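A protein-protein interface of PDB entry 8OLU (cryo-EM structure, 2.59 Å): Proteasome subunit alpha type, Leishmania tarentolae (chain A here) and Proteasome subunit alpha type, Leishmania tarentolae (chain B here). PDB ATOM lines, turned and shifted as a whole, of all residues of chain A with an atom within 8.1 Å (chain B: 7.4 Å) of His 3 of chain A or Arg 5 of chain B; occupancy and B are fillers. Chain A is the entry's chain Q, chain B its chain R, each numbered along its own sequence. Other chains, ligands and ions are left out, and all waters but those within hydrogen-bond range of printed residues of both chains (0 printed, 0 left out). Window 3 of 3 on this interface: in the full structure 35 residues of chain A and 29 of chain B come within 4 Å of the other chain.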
ATOM      1  N   SER A   2      -3.440  19.335  11.557  1.00  0.00           N
ATOM      2  CA  SER A   2      -4.585  18.733  12.282  1.00  0.00           C
ATOM      3  C   SER A   2      -4.517  17.213  12.100  1.00  0.00           C
ATOM      4  O   SER A   2      -4.767  16.520  13.084  1.00  0.00           O
ATOM      5  CB  SER A   2      -5.993  19.333  11.934  1.00  0.00           C
ATOM      6  OG  SER A   2      -6.743  19.665  13.122  1.00  0.00           O
ATOM      7  N   HIS A   3      -4.126  16.657  10.937  1.00  0.00           N
ATOM      8  CA  HIS A   3      -4.108  15.190  10.794  1.00  0.00           C
ATOM      9  C   HIS A   3      -3.151  14.483  11.777  1.00  0.00           C
ATOM     10  O   HIS A   3      -3.267  13.290  11.952  1.00  0.00           O
ATOM     11  CB  HIS A   3      -3.805  14.729   9.350  1.00  0.00           C
ATOM     12  CG  HIS A   3      -2.340  14.670   9.002  1.00  0.00           C
ATOM     13  ND1 HIS A   3      -1.585  15.775   8.648  1.00  0.00           N
ATOM     14  CD2 HIS A   3      -1.492  13.589   9.006  1.00  0.00           C
ATOM     15  CE1 HIS A   3      -0.320  15.395   8.454  1.00  0.00           C
ATOM     16  NE2 HIS A   3      -0.241  14.036   8.664  1.00  0.00           N
ATOM     17  N   ARG A   4      -2.192  15.172  12.413  1.00  0.00           N
ATOM     18  CA  ARG A   4      -1.257  14.528  13.331  1.00  0.00           C
ATOM     19  C   ARG A   4      -1.986  14.115  14.607  1.00  0.00           C
ATOM     20  O   ARG A   4      -1.488  13.308  15.378  1.00  0.00           O
ATOM     21  CB  ARG A   4      -0.113  15.464  13.753  1.00  0.00           C
ATOM     22  CG  ARG A   4       0.608  16.168  12.602  1.00  0.00           C
ATOM     23  CD  ARG A   4       1.554  17.315  12.992  1.00  0.00           C
ATOM     24  NE  ARG A   4       2.881  16.872  13.445  1.00  0.00           N
ATOM     25  CZ  ARG A   4       3.251  16.713  14.722  1.00  0.00           C
ATOM     26  NH1 ARG A   4       4.357  16.050  15.011  1.00  0.00           N
ATOM     27  NH2 ARG A   4       2.494  17.170  15.710  1.00  0.00           N
ATOM     28  N   TYR A   5      -3.149  14.727  14.826  1.00  0.00           N
ATOM     29  CA  TYR A   5      -3.891  14.634  16.068  1.00  0.00           C
ATOM     30  C   TYR A   5      -5.138  13.765  15.861  1.00  0.00           C
ATOM     31  O   TYR A   5      -6.032  13.718  16.701  1.00  0.00           O
ATOM     32  CB  TYR A   5      -4.239  16.042  16.611  1.00  0.00           C
ATOM     33  CG  TYR A   5      -3.079  17.018  16.696  1.00  0.00           C
ATOM     34  CD1 TYR A   5      -1.901  16.699  17.371  1.00  0.00           C
ATOM     35  CD2 TYR A   5      -3.114  18.237  16.028  1.00  0.00           C
ATOM     36  CE1 TYR A   5      -0.811  17.562  17.381  1.00  0.00           C
ATOM     37  CE2 TYR A   5      -2.033  19.109  16.027  1.00  0.00           C
ATOM     38  CZ  TYR A   5      -0.869  18.764  16.687  1.00  0.00           C
ATOM     39  OH  TYR A   5       0.189  19.644  16.667  1.00  0.00           O
ATOM     40  N   ASP A   6      -5.243  13.080  14.724  1.00  0.00           N
ATOM     41  CA  ASP A   6      -6.412  12.255  14.469  1.00  0.00           C
ATOM     42  C   ASP A   6      -6.115  10.935  15.156  1.00  0.00           C
ATOM     43  O   ASP A   6      -5.038  10.359  14.947  1.00  0.00           O
ATOM     44  CB  ASP A   6      -6.674  12.152  12.963  1.00  0.00           C
ATOM     45  CG  ASP A   6      -7.877  11.317  12.524  1.00  0.00           C
ATOM     46  OD1 ASP A   6      -8.511  10.734  13.381  1.00  0.00           O
ATOM     47  OD2 ASP A   6      -8.145  11.228  11.288  1.00  0.00           O
ATOM     48  N   SER A   7      -7.079  10.486  15.962  1.00  0.00           N
ATOM     49  CA  SER A   7      -6.964   9.253  16.729  1.00  0.00           C
ATOM     50  C   SER A   7      -7.487   8.026  15.967  1.00  0.00           C
ATOM     51  O   SER A   7      -7.379   6.910  16.477  1.00  0.00           O
ATOM     52  CB  SER A   7      -7.719   9.420  17.992  1.00  0.00           C
ATOM     53  OG  SER A   7      -9.082   9.778  17.691  1.00  0.00           O
ATOM     54  N   ARG A   8      -8.069   8.224  14.772  1.00  0.00           N
ATOM     55  CA  ARG A   8      -8.267   7.167  13.793  1.00  0.00           C
ATOM     56  C   ARG A   8      -9.225   6.113  14.380  1.00  0.00           C
ATOM     57  O   ARG A   8      -8.957   4.919  14.517  1.00  0.00           O
ATOM     58  CB  ARG A   8      -6.860   6.722  13.361  1.00  0.00           C
ATOM     59  CG  ARG A   8      -6.338   7.378  12.082  1.00  0.00           C
ATOM     60  CD  ARG A   8      -4.828   7.566  12.046  1.00  0.00           C
ATOM     61  NE  ARG A   8      -4.097   6.539  12.789  1.00  0.00           N
ATOM     62  CZ  ARG A   8      -3.262   6.760  13.806  1.00  0.00           C
ATOM     63  NH1 ARG A   8      -3.087   7.983  14.278  1.00  0.00           N
ATOM     64  NH2 ARG A   8      -2.611   5.742  14.350  1.00  0.00           N
ATOM     65  N   THR A  10     -12.133   4.903  13.375  1.00  0.00           N
ATOM     66  CA  THR A  10     -12.626   3.846  12.518  1.00  0.00           C
ATOM     67  C   THR A  10     -11.479   3.087  11.839  1.00  0.00           C
ATOM     68  O   THR A  10     -11.580   2.787  10.671  1.00  0.00           O
ATOM     69  CB  THR A  10     -13.591   4.421  11.470  1.00  0.00           C
ATOM     70  OG1 THR A  10     -13.006   5.294  10.495  1.00  0.00           O
ATOM     71  CG2 THR A  10     -14.705   5.211  12.115  1.00  0.00           C
ATOM     72  N   THR A  11     -10.355   2.832  12.485  1.00  0.00           N
ATOM     73  CA  THR A  11      -9.378   2.007  11.813  1.00  0.00           C
ATOM     74  C   THR A  11      -9.405   0.661  12.458  1.00  0.00           C
ATOM     75  O   THR A  11      -9.876   0.573  13.580  1.00  0.00           O
ATOM     76  CB  THR A  11      -7.911   2.443  11.944  1.00  0.00           C
ATOM     77  OG1 THR A  11      -7.500   2.674  13.297  1.00  0.00           O
ATOM     78  CG2 THR A  11      -7.667   3.681  11.116  1.00  0.00           C
ATOM     79  N   GLY A 131     -16.526   8.111   9.251  1.00  0.00           N
ATOM     80  CA  GLY A 131     -16.887   9.372   9.894  1.00  0.00           C
ATOM     81  C   GLY A 131     -15.821   9.860  10.857  1.00  0.00           C
ATOM     82  O   GLY A 131     -15.857  11.008  11.297  1.00  0.00           O
ATOM     83  N   GLY A 132     -14.862   8.993  11.165  1.00  0.00           N
ATOM     84  CA  GLY A 132     -13.775   9.433  12.030  1.00  0.00           C
ATOM     85  C   GLY A 132     -14.145   9.942  13.430  1.00  0.00           C
ATOM     86  O   GLY A 132     -13.236  10.323  14.137  1.00  0.00           O
ATOM     87  N   SER B   2     -17.011  16.768   5.181  1.00  0.00           N
ATOM     88  CA  SER B   2     -17.012  15.295   5.480  1.00  0.00           C
ATOM     89  C   SER B   2     -15.598  14.818   5.816  1.00  0.00           C
ATOM     90  O   SER B   2     -14.600  15.357   5.324  1.00  0.00           O
ATOM     91  CB  SER B   2     -17.576  14.467   4.320  1.00  0.00           C
ATOM     92  OG  SER B   2     -18.469  13.440   4.764  1.00  0.00           O
ATOM     93  N   TYR B   3     -15.521  13.811   6.698  1.00  0.00           N
ATOM     94  CA  TYR B   3     -14.240  13.218   7.030  1.00  0.00           C
ATOM     95  C   TYR B   3     -13.856  12.267   5.918  1.00  0.00           C
ATOM     96  O   TYR B   3     -14.646  11.376   5.604  1.00  0.00           O
ATOM     97  CB  TYR B   3     -14.325  12.404   8.296  1.00  0.00           C
ATOM     98  CG  TYR B   3     -13.060  11.725   8.747  1.00  0.00           C
ATOM     99  CD1 TYR B   3     -12.041  12.412   9.369  1.00  0.00           C
ATOM    100  CD2 TYR B   3     -12.919  10.363   8.666  1.00  0.00           C
ATOM    101  CE1 TYR B   3     -10.923  11.767   9.890  1.00  0.00           C
ATOM    102  CE2 TYR B   3     -11.790   9.715   9.145  1.00  0.00           C
ATOM    103  CZ  TYR B   3     -10.804  10.407   9.796  1.00  0.00           C
ATOM    104  OH  TYR B   3      -9.696   9.731  10.231  1.00  0.00           O
ATOM    105  N   ASP B   4     -12.676  12.519   5.332  1.00  0.00           N
ATOM    106  CA  ASP B   4     -12.223  11.800   4.159  1.00  0.00           C
ATOM    107  C   ASP B   4     -10.760  11.514   4.297  1.00  0.00           C
ATOM    108  O   ASP B   4     -10.128  11.291   3.299  1.00  0.00           O
ATOM    109  CB  ASP B   4     -12.428  12.548   2.827  1.00  0.00           C
ATOM    110  CG  ASP B   4     -11.835  13.962   2.709  1.00  0.00           C
ATOM    111  OD1 ASP B   4     -10.582  14.109   2.817  1.00  0.00           O
ATOM    112  OD2 ASP B   4     -12.626  14.935   2.468  1.00  0.00           O
ATOM    113  N   ARG B   5     -10.237  11.412   5.504  1.00  0.00           N
ATOM    114  CA  ARG B   5      -8.862  10.971   5.605  1.00  0.00           C
ATOM    115  C   ARG B   5      -8.697   9.617   4.933  1.00  0.00           C
ATOM    116  O   ARG B   5      -9.638   8.838   4.809  1.00  0.00           O
ATOM    117  CB  ARG B   5      -8.373  10.802   7.035  1.00  0.00           C
ATOM    118  CG  ARG B   5      -6.864  10.971   7.158  1.00  0.00           C
ATOM    119  CD  ARG B   5      -6.475  10.694   8.593  1.00  0.00           C
ATOM    120  NE  ARG B   5      -5.066  10.912   8.880  1.00  0.00           N
ATOM    121  CZ  ARG B   5      -4.338  10.068   9.592  1.00  0.00           C
ATOM    122  NH1 ARG B   5      -4.580   8.770   9.503  1.00  0.00           N
ATOM    123  NH2 ARG B   5      -3.391  10.520  10.395  1.00  0.00           N
ATOM    124  N   ALA B   6      -7.466   9.351   4.526  1.00  0.00           N
ATOM    125  CA  ALA B   6      -7.120   8.122   3.860  1.00  0.00           C
ATOM    126  C   ALA B   6      -6.738   7.100   4.909  1.00  0.00           C
ATOM    127  O   ALA B   6      -5.628   7.173   5.427  1.00  0.00           O
ATOM    128  CB  ALA B   6      -5.969   8.358   2.895  1.00  0.00           C
ATOM    129  N   ILE B   7      -7.610   6.100   5.085  1.00  0.00           N
ATOM    130  CA  ILE B   7      -7.463   5.091   6.116  1.00  0.00           C
ATOM    131  C   ILE B   7      -6.662   3.904   5.589  1.00  0.00           C
ATOM    132  O   ILE B   7      -5.688   3.474   6.183  1.00  0.00           O
ATOM    133  CB  ILE B   7      -8.855   4.704   6.617  1.00  0.00           C
ATOM    134  CG1 ILE B   7      -9.422   5.823   7.493  1.00  0.00           C
ATOM    135  CG2 ILE B   7      -8.828   3.395   7.363  1.00  0.00           C
ATOM    136  CD1 ILE B   7     -10.928   5.743   7.701  1.00  0.00           C
ATOM    137  N   THR B   8      -7.039   3.444   4.418  1.00  0.00           N
ATOM    138  CA  THR B   8      -6.373   2.350   3.764  1.00  0.00           C
ATOM    139  C   THR B   8      -5.283   2.925   2.866  1.00  0.00           C
ATOM    140  O   THR B   8      -5.590   3.586   1.876  1.00  0.00           O
ATOM    141  CB  THR B   8      -7.396   1.520   2.971  1.00  0.00           C
ATOM    142  OG1 THR B   8      -8.584   1.251   3.731  1.00  0.00           O
ATOM    143  CG2 THR B   8      -6.808   0.198   2.508  1.00  0.00           C
ATOM    144  N   VAL B   9      -4.025   2.620   3.183  1.00  0.00           N
ATOM    145  CA  VAL B   9      -2.905   3.141   2.419  1.00  0.00           C
ATOM    146  C   VAL B   9      -1.833   2.084   2.307  1.00  0.00           C
ATOM    147  O   VAL B   9      -1.723   1.222   3.168  1.00  0.00           O
ATOM    148  CB  VAL B   9      -2.313   4.366   3.134  1.00  0.00           C
ATOM    149  CG1 VAL B   9      -3.332   5.468   3.218  1.00  0.00           C
ATOM    150  CG2 VAL B   9      -1.845   4.055   4.535  1.00  0.00           C
ATOM    151  N   SER B 121     -11.833   4.168  -0.220  1.00  0.00           N
ATOM    152  CA  SER B 121     -12.625   5.352   0.040  1.00  0.00           C
ATOM    153  C   SER B 121     -12.048   5.999   1.272  1.00  0.00           C
ATOM    154  O   SER B 121     -11.816   5.354   2.296  1.00  0.00           O
ATOM    155  CB  SER B 121     -14.130   5.052   0.231  1.00  0.00           C
ATOM    156  OG  SER B 121     -14.362   4.402   1.485  1.00  0.00           O
ATOM    157  N   GLY B 122     -11.772   7.276   1.131  1.00  0.00           N
ATOM    158  CA  GLY B 122     -11.292   8.020   2.269  1.00  0.00           C
ATOM    159  C   GLY B 122     -12.456   8.186   3.230  1.00  0.00           C
ATOM    160  O   GLY B 122     -13.562   8.529   2.820  1.00  0.00           O
ATOM    161  N   GLY B 123     -12.140   7.928   4.498  1.00  0.00           N
ATOM    162  CA  GLY B 123     -13.059   8.175   5.575  1.00  0.00           C
ATOM    163  C   GLY B 123     -13.533   6.869   6.185  1.00  0.00           C
ATOM    164  O   GLY B 123     -14.038   6.856   7.318  1.00  0.00           O
ATOM    165  N   SER B 124     -13.322   5.775   5.442  1.00  0.00           N
ATOM    166  CA  SER B 124     -13.961   4.523   5.787  1.00  0.00           C
ATOM    167  C   SER B 124     -12.900   3.452   5.983  1.00  0.00           C
ATOM    168  O   SER B 124     -11.886   3.446   5.279  1.00  0.00           O
ATOM    169  CB  SER B 124     -14.997   4.177   4.719  1.00  0.00           C
ATOM    170  OG  SER B 124     -14.795   2.862   4.156  1.00  0.00           O
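The backbone carbonyl oxygen (O) of His 3 of chain A sits at hydrogen-bond distance from the guanidinium group (NH2) of Arg 5 of chain B (3.2 Å).
OD2 of Asp 6 of chain A is in hydrogen-bond range of OH of Tyr 3 of chain B (2.4 Å).
The backbone carbonyl oxygen (O) of Gly 123 of chain B lies within hydrogen-bond range of the backbone NH (N) of Gly 131 of chain A.
The guanidinium group (NE) of Arg 5 of chain B is in salt-bridge range of the side-chain carboxylate (OD2) of Asp 6 of chain A (3.9 Å).
The backbone carbonyl oxygen of Arg 8 of chain A is in hydrogen-bond range of the side-chain hydroxyl of Thr 11 of chain A, at 2.9 Å.
O of Arg 5 of chain B is in hydrogen-bond range of N of Gly 123 of chain B, 2.7 Å away.
The side-chain carboxylate of Asp 6 of chain A lies within hydrogen-bond range of the backbone NH of Arg 8 of chain A.
Arg 8 of chain A touches Arg 5 of chain B (CD to NH1, 2.8 Å).
Thr 10 of chain A touches Ile 7 of chain B.
OG1 of Thr 10 of chain A touches O of Gly 123 of chain B, at 3.7 Å.
Thr 11 of chain A touches Ile 7 of chain B.
Gly 131 of chain A touches Tyr 3 of chain B.
Gly 132 of chain A touches Tyr 3 of chain B.
His 3 of chain A touches one residue of chain B.
Of the printed residues of chain A, Arg 5 of chain B touches His 3, Asp 6 and Arg 8.
Of the printed residues of chain B, Asp 6 of chain A touches Tyr 3 (2.4 Å) and Arg 5 (3.2 Å).
Printed residues of chain A within 4 Å of Gly 123 of chain B: Thr 10 (3.7 Å) and Gly 131 (3.4 Å).
Of the printed residues of chain B, Gly 132 of chain A touches Tyr 3 (3.4 Å).
Of the printed residues of chain A, Tyr 3 of chain B touches Asp 6, Gly 131 and Gly 132.
Asp 4 of chain B touches none of the printed residues of chain A.
The nearest printed residue of chain B that does not touch His 3 of chain A is Tyr 3 of chain B (7.5 Å).
The nearest residue of chain A that does not touch Arg 5 of chain B is Arg 4 of chain A (5.2 Å).
Printed residues of chain B that touch a printed residue of chain A: Tyr 3, Arg 5, Ile 7 and Gly 123.
Hydrophobic or aromatic side chains of chain A within 4 Å of the printed part of chain B: His 3.
Among the printed residues, Asp or Glu carboxylates within 4 Å of a Lys or Arg side-chain nitrogen of the other chain: Asp 6 of chain A with Arg 5 of chain B (3.9 Å).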
